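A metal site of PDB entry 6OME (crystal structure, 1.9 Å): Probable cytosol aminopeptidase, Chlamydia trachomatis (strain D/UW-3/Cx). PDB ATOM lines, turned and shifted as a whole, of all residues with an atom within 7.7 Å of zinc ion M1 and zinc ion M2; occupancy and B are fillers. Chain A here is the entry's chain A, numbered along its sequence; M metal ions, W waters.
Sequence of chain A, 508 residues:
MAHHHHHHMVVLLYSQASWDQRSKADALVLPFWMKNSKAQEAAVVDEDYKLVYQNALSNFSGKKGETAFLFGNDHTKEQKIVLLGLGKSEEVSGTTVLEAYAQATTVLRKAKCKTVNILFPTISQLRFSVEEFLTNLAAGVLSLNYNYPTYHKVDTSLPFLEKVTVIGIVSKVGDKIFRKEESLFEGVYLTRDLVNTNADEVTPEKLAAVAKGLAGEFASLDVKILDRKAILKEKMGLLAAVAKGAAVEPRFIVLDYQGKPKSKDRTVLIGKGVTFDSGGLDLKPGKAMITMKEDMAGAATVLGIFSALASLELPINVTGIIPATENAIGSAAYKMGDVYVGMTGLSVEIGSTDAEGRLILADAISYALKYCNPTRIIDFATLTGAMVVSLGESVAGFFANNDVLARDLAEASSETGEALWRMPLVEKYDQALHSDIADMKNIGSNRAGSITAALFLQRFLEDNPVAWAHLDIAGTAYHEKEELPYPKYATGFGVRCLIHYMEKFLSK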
ATOM      1  N   LYS A 272       2.297 -10.961  -6.029  1.00  0.00           N
ATOM      2  CA  LYS A 272       2.676  -9.547  -5.942  1.00  0.00           C
ATOM      3  C   LYS A 272       4.152  -9.417  -5.575  1.00  0.00           C
ATOM      4  O   LYS A 272       4.581  -9.907  -4.527  1.00  0.00           O
ATOM      5  CB  LYS A 272       1.795  -8.846  -4.909  1.00  0.00           C
ATOM      6  CG  LYS A 272       2.299  -7.443  -4.532  1.00  0.00           C
ATOM      7  CD  LYS A 272       1.450  -6.776  -3.423  1.00  0.00           C
ATOM      8  CE  LYS A 272       2.152  -5.471  -2.905  1.00  0.00           C
ATOM      9  NZ  LYS A 272       1.347  -4.708  -1.898  1.00  0.00           N
ATOM     10  N   GLY A 273       4.928  -8.777  -6.445  1.00  0.00           N
ATOM     11  CA  GLY A 273       6.348  -8.612  -6.196  1.00  0.00           C
ATOM     12  C   GLY A 273       6.806  -7.173  -6.004  1.00  0.00           C
ATOM     13  O   GLY A 273       7.683  -6.709  -6.734  1.00  0.00           O
ATOM     14  N   VAL A 274       6.251  -6.464  -5.032  1.00  0.00           N
ATOM     15  CA  VAL A 274       6.740  -5.113  -4.735  1.00  0.00           C
ATOM     16  C   VAL A 274       7.936  -5.265  -3.816  1.00  0.00           C
ATOM     17  O   VAL A 274       7.791  -5.603  -2.640  1.00  0.00           O
ATOM     18  CB  VAL A 274       5.657  -4.230  -4.113  1.00  0.00           C
ATOM     19  CG1 VAL A 274       6.248  -2.881  -3.692  1.00  0.00           C
ATOM     20  CG2 VAL A 274       4.542  -3.994  -5.154  1.00  0.00           C
ATOM     21  N   THR A 275       9.135  -5.072  -4.363  1.00  0.00           N
ATOM     22  CA  THR A 275      10.336  -5.483  -3.640  1.00  0.00           C
ATOM     23  C   THR A 275      10.660  -4.522  -2.499  1.00  0.00           C
ATOM     24  O   THR A 275      11.399  -4.899  -1.582  1.00  0.00           O
ATOM     25  CB  THR A 275      11.513  -5.614  -4.608  1.00  0.00           C
ATOM     26  OG1 THR A 275      11.660  -4.398  -5.352  1.00  0.00           O
ATOM     27  CG2 THR A 275      11.254  -6.771  -5.597  1.00  0.00           C
ATOM     28  N   PHE A 276      10.115  -3.307  -2.532  1.00  0.00           N
ATOM     29  CA  PHE A 276      10.083  -2.446  -1.356  1.00  0.00           C
ATOM     30  C   PHE A 276       8.957  -1.437  -1.581  1.00  0.00           C
ATOM     31  O   PHE A 276       8.881  -0.828  -2.644  1.00  0.00           O
ATOM     32  CB  PHE A 276      11.414  -1.710  -1.123  1.00  0.00           C
ATOM     33  CG  PHE A 276      11.436  -0.876   0.144  1.00  0.00           C
ATOM     34  CD1 PHE A 276      11.740  -1.458   1.383  1.00  0.00           C
ATOM     35  CD2 PHE A 276      11.123   0.480   0.106  1.00  0.00           C
ATOM     36  CE1 PHE A 276      11.743  -0.693   2.557  1.00  0.00           C
ATOM     37  CE2 PHE A 276      11.120   1.249   1.275  1.00  0.00           C
ATOM     38  CZ  PHE A 276      11.435   0.666   2.497  1.00  0.00           C
ATOM     39  N   ASP A 277       8.097  -1.272  -0.584  1.00  0.00           N
ATOM     40  CA  ASP A 277       6.932  -0.407  -0.665  1.00  0.00           C
ATOM     41  C   ASP A 277       7.123   0.788   0.260  1.00  0.00           C
ATOM     42  O   ASP A 277       6.897   0.685   1.468  1.00  0.00           O
ATOM     43  CB  ASP A 277       5.683  -1.206  -0.323  1.00  0.00           C
ATOM     44  CG  ASP A 277       4.407  -0.459  -0.622  1.00  0.00           C
ATOM     45  OD1 ASP A 277       4.436   0.700  -1.101  1.00  0.00           O
ATOM     46  OD2 ASP A 277       3.367  -1.075  -0.406  1.00  0.00           O
ATOM     47  N   SER A 278       7.560   1.930  -0.292  1.00  0.00           N
ATOM     48  CA  SER A 278       7.597   3.173   0.467  1.00  0.00           C
ATOM     49  C   SER A 278       6.207   3.768   0.656  1.00  0.00           C
ATOM     50  O   SER A 278       6.043   4.665   1.498  1.00  0.00           O
ATOM     51  CB  SER A 278       8.459   4.227  -0.227  1.00  0.00           C
ATOM     52  OG  SER A 278       7.807   4.636  -1.431  1.00  0.00           O
ATOM     53  N   GLY A 279       5.231   3.323  -0.124  1.00  0.00           N
ATOM     54  CA  GLY A 279       3.934   3.958  -0.218  1.00  0.00           C
ATOM     55  C   GLY A 279       3.805   4.916  -1.388  1.00  0.00           C
ATOM     56  O   GLY A 279       2.683   5.260  -1.775  1.00  0.00           O
ATOM     57  N   GLY A 280       4.928   5.342  -1.986  1.00  0.00           N
ATOM     58  CA  GLY A 280       4.893   6.342  -3.054  1.00  0.00           C
ATOM     59  C   GLY A 280       4.668   7.730  -2.498  1.00  0.00           C
ATOM     60  O   GLY A 280       4.952   8.021  -1.339  1.00  0.00           O
ATOM     61  N   ASP A 282       2.019   9.012  -1.487  1.00  0.00           N
ATOM     62  CA  ASP A 282       1.282   8.789  -0.230  1.00  0.00           C
ATOM     63  C   ASP A 282       2.178   8.008   0.725  1.00  0.00           C
ATOM     64  O   ASP A 282       1.949   6.839   1.046  1.00  0.00           O
ATOM     65  CB  ASP A 282      -0.019   8.040  -0.514  1.00  0.00           C
ATOM     66  CG  ASP A 282      -1.010   8.112   0.644  1.00  0.00           C
ATOM     67  OD1 ASP A 282      -0.706   8.800   1.646  1.00  0.00           O
ATOM     68  OD2 ASP A 282      -2.090   7.491   0.558  1.00  0.00           O
ATOM     69  N   LYS A 284       4.393   6.170   3.400  1.00  0.00           N
ATOM     70  CA  LYS A 284       4.089   5.478   4.653  1.00  0.00           C
ATOM     71  C   LYS A 284       4.798   6.154   5.827  1.00  0.00           C
ATOM     72  O   LYS A 284       5.924   6.642   5.684  1.00  0.00           O
ATOM     73  CB  LYS A 284       4.549   4.022   4.584  1.00  0.00           C
ATOM     74  CG  LYS A 284       3.760   3.115   3.658  1.00  0.00           C
ATOM     75  CD  LYS A 284       4.402   1.701   3.705  1.00  0.00           C
ATOM     76  CE  LYS A 284       3.660   0.710   2.795  1.00  0.00           C
ATOM     77  NZ  LYS A 284       2.231   0.592   3.168  1.00  0.00           N
ATOM     78  N   MET A 292       8.941  -3.317   5.029  1.00  0.00           N
ATOM     79  CA  MET A 292       8.348  -3.402   3.690  1.00  0.00           C
ATOM     80  C   MET A 292       9.241  -4.074   2.650  1.00  0.00           C
ATOM     81  O   MET A 292       8.840  -4.134   1.473  1.00  0.00           O
ATOM     82  CB  MET A 292       7.916  -2.024   3.216  1.00  0.00           C
ATOM     83  CG  MET A 292       6.606  -1.577   3.873  1.00  0.00           C
ATOM     84  SD  MET A 292       5.214  -2.682   3.506  1.00  0.00           S
ATOM     85  CE  MET A 292       5.043  -3.569   5.046  1.00  0.00           C
ATOM     86  N   GLU A 294       9.087  -7.018   2.911  1.00  0.00           N
ATOM     87  CA  GLU A 294       8.194  -8.176   2.836  1.00  0.00           C
ATOM     88  C   GLU A 294       7.159  -8.056   1.740  1.00  0.00           C
ATOM     89  O   GLU A 294       6.426  -9.026   1.480  1.00  0.00           O
ATOM     90  CB  GLU A 294       7.472  -8.380   4.164  1.00  0.00           C
ATOM     91  CG  GLU A 294       6.351  -7.342   4.435  1.00  0.00           C
ATOM     92  CD  GLU A 294       5.493  -7.740   5.620  1.00  0.00           C
ATOM     93  OE1 GLU A 294       4.628  -8.625   5.454  1.00  0.00           O
ATOM     94  OE2 GLU A 294       5.715  -7.222   6.725  1.00  0.00           O
ATOM     95  N   ASP A 295       7.066  -6.896   1.086  1.00  0.00           N
ATOM     96  CA  ASP A 295       5.919  -6.655   0.220  1.00  0.00           C
ATOM     97  C   ASP A 295       6.012  -7.418  -1.095  1.00  0.00           C
ATOM     98  O   ASP A 295       5.115  -7.283  -1.931  1.00  0.00           O
ATOM     99  CB  ASP A 295       5.783  -5.144  -0.038  1.00  0.00           C
ATOM    100  CG  ASP A 295       4.336  -4.720  -0.271  1.00  0.00           C
ATOM    101  OD1 ASP A 295       3.402  -5.296   0.341  1.00  0.00           O
ATOM    102  OD2 ASP A 295       4.150  -3.793  -1.083  1.00  0.00           O
ATOM    103  N   MET A 296       7.061  -8.227  -1.277  1.00  0.00           N
ATOM    104  CA  MET A 296       7.175  -9.111  -2.429  1.00  0.00           C
ATOM    105  C   MET A 296       6.930 -10.554  -2.033  1.00  0.00           C
ATOM    106  O   MET A 296       7.265 -11.473  -2.799  1.00  0.00           O
ATOM    107  CB  MET A 296       8.534  -8.943  -3.130  1.00  0.00           C
ATOM    108  CG  MET A 296       9.755  -8.800  -2.207  1.00  0.00           C
ATOM    109  SD  MET A 296       9.993 -10.165  -1.033  1.00  0.00           S
ATOM    110  CE  MET A 296      10.543 -11.471  -2.153  1.00  0.00           C
ATOM    111  N   ASN A 327       8.028   0.350  -5.164  1.00  0.00           N
ATOM    112  CA  ASN A 327       7.065   1.462  -5.120  1.00  0.00           C
ATOM    113  C   ASN A 327       7.796   2.606  -4.430  1.00  0.00           C
ATOM    114  O   ASN A 327       7.842   2.710  -3.205  1.00  0.00           O
ATOM    115  CB  ASN A 327       5.788   1.090  -4.354  1.00  0.00           C
ATOM    116  CG  ASN A 327       4.693   2.158  -4.513  1.00  0.00           C
ATOM    117  OD1 ASN A 327       4.662   2.906  -5.493  1.00  0.00           O
ATOM    118  ND2 ASN A 327       3.776   2.222  -3.548  1.00  0.00           N
ATOM    119  N   TYR A 334       4.451   7.905  -9.745  1.00  0.00           N
ATOM    120  CA  TYR A 334       3.107   8.068 -10.302  1.00  0.00           C
ATOM    121  C   TYR A 334       2.233   8.822  -9.306  1.00  0.00           C
ATOM    122  O   TYR A 334       2.457   8.797  -8.088  1.00  0.00           O
ATOM    123  CB  TYR A 334       2.499   6.717 -10.685  1.00  0.00           C
ATOM    124  CG  TYR A 334       1.931   5.826  -9.582  1.00  0.00           C
ATOM    125  CD1 TYR A 334       2.729   5.342  -8.538  1.00  0.00           C
ATOM    126  CD2 TYR A 334       0.598   5.416  -9.621  1.00  0.00           C
ATOM    127  CE1 TYR A 334       2.188   4.480  -7.553  1.00  0.00           C
ATOM    128  CE2 TYR A 334       0.054   4.566  -8.677  1.00  0.00           C
ATOM    129  CZ  TYR A 334       0.854   4.105  -7.634  1.00  0.00           C
ATOM    130  OH  TYR A 334       0.265   3.271  -6.712  1.00  0.00           O
ATOM    131  N   SER A 352      -4.909   6.352  -3.791  1.00  0.00           N
ATOM    132  CA  SER A 352      -3.688   6.297  -2.986  1.00  0.00           C
ATOM    133  C   SER A 352      -2.607   5.539  -3.732  1.00  0.00           C
ATOM    134  O   SER A 352      -2.828   4.423  -4.203  1.00  0.00           O
ATOM    135  CB  SER A 352      -3.927   5.613  -1.624  1.00  0.00           C
ATOM    136  OG  SER A 352      -2.663   5.387  -0.984  1.00  0.00           O
ATOM    137  N   THR A 353      -1.423   6.150  -3.844  1.00  0.00           N
ATOM    138  CA  THR A 353      -0.290   5.440  -4.432  1.00  0.00           C
ATOM    139  C   THR A 353       0.176   4.263  -3.569  1.00  0.00           C
ATOM    140  O   THR A 353       0.968   3.441  -4.060  1.00  0.00           O
ATOM    141  CB  THR A 353       0.872   6.398  -4.653  1.00  0.00           C
ATOM    142  OG1 THR A 353       1.297   6.913  -3.386  1.00  0.00           O
ATOM    143  CG2 THR A 353       0.454   7.565  -5.567  1.00  0.00           C
ATOM    144  N   ASP A 354      -0.248   4.185  -2.308  1.00  0.00           N
ATOM    145  CA  ASP A 354       0.067   3.054  -1.434  1.00  0.00           C
ATOM    146  C   ASP A 354      -0.852   1.864  -1.686  1.00  0.00           C
ATOM    147  O   ASP A 354      -0.708   0.835  -1.019  1.00  0.00           O
ATOM    148  CB  ASP A 354      -0.003   3.503   0.037  1.00  0.00           C
ATOM    149  CG  ASP A 354       0.774   2.583   1.004  1.00  0.00           C
ATOM    150  OD1 ASP A 354       1.606   1.774   0.565  1.00  0.00           O
ATOM    151  OD2 ASP A 354       0.565   2.695   2.230  1.00  0.00           O
ATOM    152  N   ALA A 355      -1.837   1.994  -2.561  1.00  0.00           N
ATOM    153  CA  ALA A 355      -2.608   0.834  -3.031  1.00  0.00           C
ATOM    154  C   ALA A 355      -2.078   0.386  -4.390  1.00  0.00           C
ATOM    155  O   ALA A 355      -2.815   0.325  -5.378  1.00  0.00           O
ATOM    156  CB  ALA A 355      -4.094   1.175  -3.087  1.00  0.00           C
ATOM    157  N   GLU A 356      -0.768   0.125  -4.444  1.00  0.00           N
ATOM    158  CA  GLU A 356      -0.062  -0.156  -5.678  1.00  0.00           C
ATOM    159  C   GLU A 356      -0.073  -1.641  -6.038  1.00  0.00           C
ATOM    160  O   GLU A 356       0.011  -1.980  -7.210  1.00  0.00           O
ATOM    161  CB  GLU A 356       1.409   0.336  -5.596  1.00  0.00           C
ATOM    162  CG  GLU A 356       2.414  -0.709  -5.009  1.00  0.00           C
ATOM    163  CD  GLU A 356       2.148  -1.064  -3.547  1.00  0.00           C
ATOM    164  OE1 GLU A 356       1.496  -0.248  -2.854  1.00  0.00           O
ATOM    165  OE2 GLU A 356       2.593  -2.146  -3.053  1.00  0.00           O
ATOM    166  N   GLY A 357      -0.163  -2.519  -5.034  1.00  0.00           N
ATOM    167  CA  GLY A 357      -0.080  -3.940  -5.330  1.00  0.00           C
ATOM    168  C   GLY A 357      -1.234  -4.417  -6.188  1.00  0.00           C
ATOM    169  O   GLY A 357      -1.053  -5.223  -7.100  1.00  0.00           O
ATOM    170  N   ARG A 358      -2.442  -3.894  -5.923  1.00  0.00           N
ATOM    171  CA  ARG A 358      -3.593  -4.323  -6.707  1.00  0.00           C
ATOM    172  C   ARG A 358      -3.457  -3.874  -8.160  1.00  0.00           C
ATOM    173  O   ARG A 358      -3.961  -4.549  -9.061  1.00  0.00           O
ATOM    174  CB  ARG A 358      -4.888  -3.771  -6.086  1.00  0.00           C
ATOM    175  CG  ARG A 358      -5.024  -2.265  -6.108  1.00  0.00           C
ATOM    176  CD  ARG A 358      -6.127  -1.819  -5.127  1.00  0.00           C
ATOM    177  NE  ARG A 358      -5.647  -1.995  -3.760  1.00  0.00           N
ATOM    178  CZ  ARG A 358      -6.381  -1.741  -2.679  1.00  0.00           C
ATOM    179  NH1 ARG A 358      -7.623  -1.304  -2.814  1.00  0.00           N
ATOM    180  NH2 ARG A 358      -5.871  -1.938  -1.461  1.00  0.00           N
ATOM    181  N   ILE A 360      -0.547  -3.715  -9.939  1.00  0.00           N
ATOM    182  CA  ILE A 360       0.332  -4.586 -10.711  1.00  0.00           C
ATOM    183  C   ILE A 360      -0.278  -5.967 -10.845  1.00  0.00           C
ATOM    184  O   ILE A 360      -0.051  -6.659 -11.845  1.00  0.00           O
ATOM    185  CB  ILE A 360       1.755  -4.613 -10.121  1.00  0.00           C
ATOM    186  CG1 ILE A 360       1.847  -5.494  -8.873  1.00  0.00           C
ATOM    187  CG2 ILE A 360       2.250  -3.198  -9.776  1.00  0.00           C
ATOM    188  CD1 ILE A 360       3.251  -5.512  -8.286  1.00  0.00           C
ATOM    189  N   THR A 382       0.708  -9.600  -0.217  1.00  0.00           N
ATOM    190  CA  THR A 382       0.686  -8.818   1.023  1.00  0.00           C
ATOM    191  C   THR A 382      -0.078  -7.531   0.726  1.00  0.00           C
ATOM    192  O   THR A 382       0.497  -6.462   0.503  1.00  0.00           O
ATOM    193  CB  THR A 382       2.092  -8.526   1.510  1.00  0.00           C
ATOM    194  OG1 THR A 382       2.851  -7.979   0.414  1.00  0.00           O
ATOM    195  CG2 THR A 382       2.790  -9.781   2.029  1.00  0.00           C
ATOM    196  N   LEU A 383      -1.400  -7.636   0.680  1.00  0.00           N
ATOM    197  CA  LEU A 383      -2.158  -6.598   0.013  1.00  0.00           C
ATOM    198  C   LEU A 383      -2.665  -5.504   0.948  1.00  0.00           C
ATOM    199  O   LEU A 383      -2.496  -4.321   0.643  1.00  0.00           O
ATOM    200  CB  LEU A 383      -3.344  -7.204  -0.770  1.00  0.00           C
ATOM    201  CG  LEU A 383      -3.849  -6.304  -1.898  1.00  0.00           C
ATOM    202  CD1 LEU A 383      -2.725  -6.047  -2.901  1.00  0.00           C
ATOM    203  CD2 LEU A 383      -5.077  -6.895  -2.614  1.00  0.00           C
ATOM    204  N   THR A 384      -3.329  -5.841   2.068  1.00  0.00           N
ATOM    205  CA  THR A 384      -3.997  -4.783   2.828  1.00  0.00           C
ATOM    206  C   THR A 384      -3.717  -4.859   4.314  1.00  0.00           C
ATOM    207  O   THR A 384      -3.758  -5.941   4.913  1.00  0.00           O
ATOM    208  CB  THR A 384      -5.544  -4.808   2.624  1.00  0.00           C
ATOM    209  OG1 THR A 384      -6.070  -6.073   3.073  1.00  0.00           O
ATOM    210  CG2 THR A 384      -5.889  -4.610   1.141  1.00  0.00           C
HETATM  211 ZN    ZN M   1       1.439  -0.122  -0.689  1.00  0.00          ZN
HETATM  212 ZN    ZN M   2       2.417  -2.965  -1.374  1.00  0.00          ZN
HETATM  213  O   HOH W   1       1.051  -2.012   1.998  1.00  0.00           O
HETATM  214  O   HOH W   2       0.738  -2.310  -0.397  1.00  0.00           O
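The nearest printed residue that does not touch zinc ion M2 is Thr 382 (4.4 Å).
Zinc ion M1 is bound by the side-chain carboxylate (OD2) of Asp 277, the side-chain carboxylate (OE1) of Glu 356, the side-chain carboxylate (OD1) of Asp 354, water W2 and the backbone carbonyl oxygen (O) of Asp 354.
Within 4 Å of zinc ion M1: Asp 277, Asp 354 and Glu 356.
The nearest printed residue that does not touch zinc ion M1 is Lys 284 (4.002 Å).
N of Asp 354 is in hydrogen-bond range of O of Gly 279, at 3.2 Å.
N of Asp 354 lies within hydrogen-bond range of OG of Ser 352 (3.0 Å).
The side-chain amide nitrogen (ND2) of Asn 327 lies close to the side-chain carboxylate (OE1) of Glu 356 (3.4 Å).
OD1 of Asp 277 sits at hydrogen-bond distance from ND2 of Asn 327, at 3.0 Å.
NZ of Lys 284 is in salt-bridge range of OD2 of Asp 354.
The side-chain amino group (NZ) of Lys 272 lies close to the backbone carbonyl oxygen (O) of Thr 382 (3.1 Å).
The backbone NH of Gly 279 lies within hydrogen-bond range of the side-chain carboxylate of Asp 277 (2.9 Å).
O of Asp 295 lies within hydrogen-bond range of N of Val 274, 3.4 Å away.
Zinc ion M2 is bound by OE2 of Glu 356 (1.9 Å).
Zinc ion M2 is bound by OD2 of Asp 295 (1.9 Å).
Zinc ion M2 is bound by water W2 (2.1 Å).
NZ of Lys 272 is bound to zinc ion M2 (2.1 Å).
OD2 of Asp 277 binds zinc ion M2 (2.3 Å).
Zinc ion M2 has five donor atoms within binding distance.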
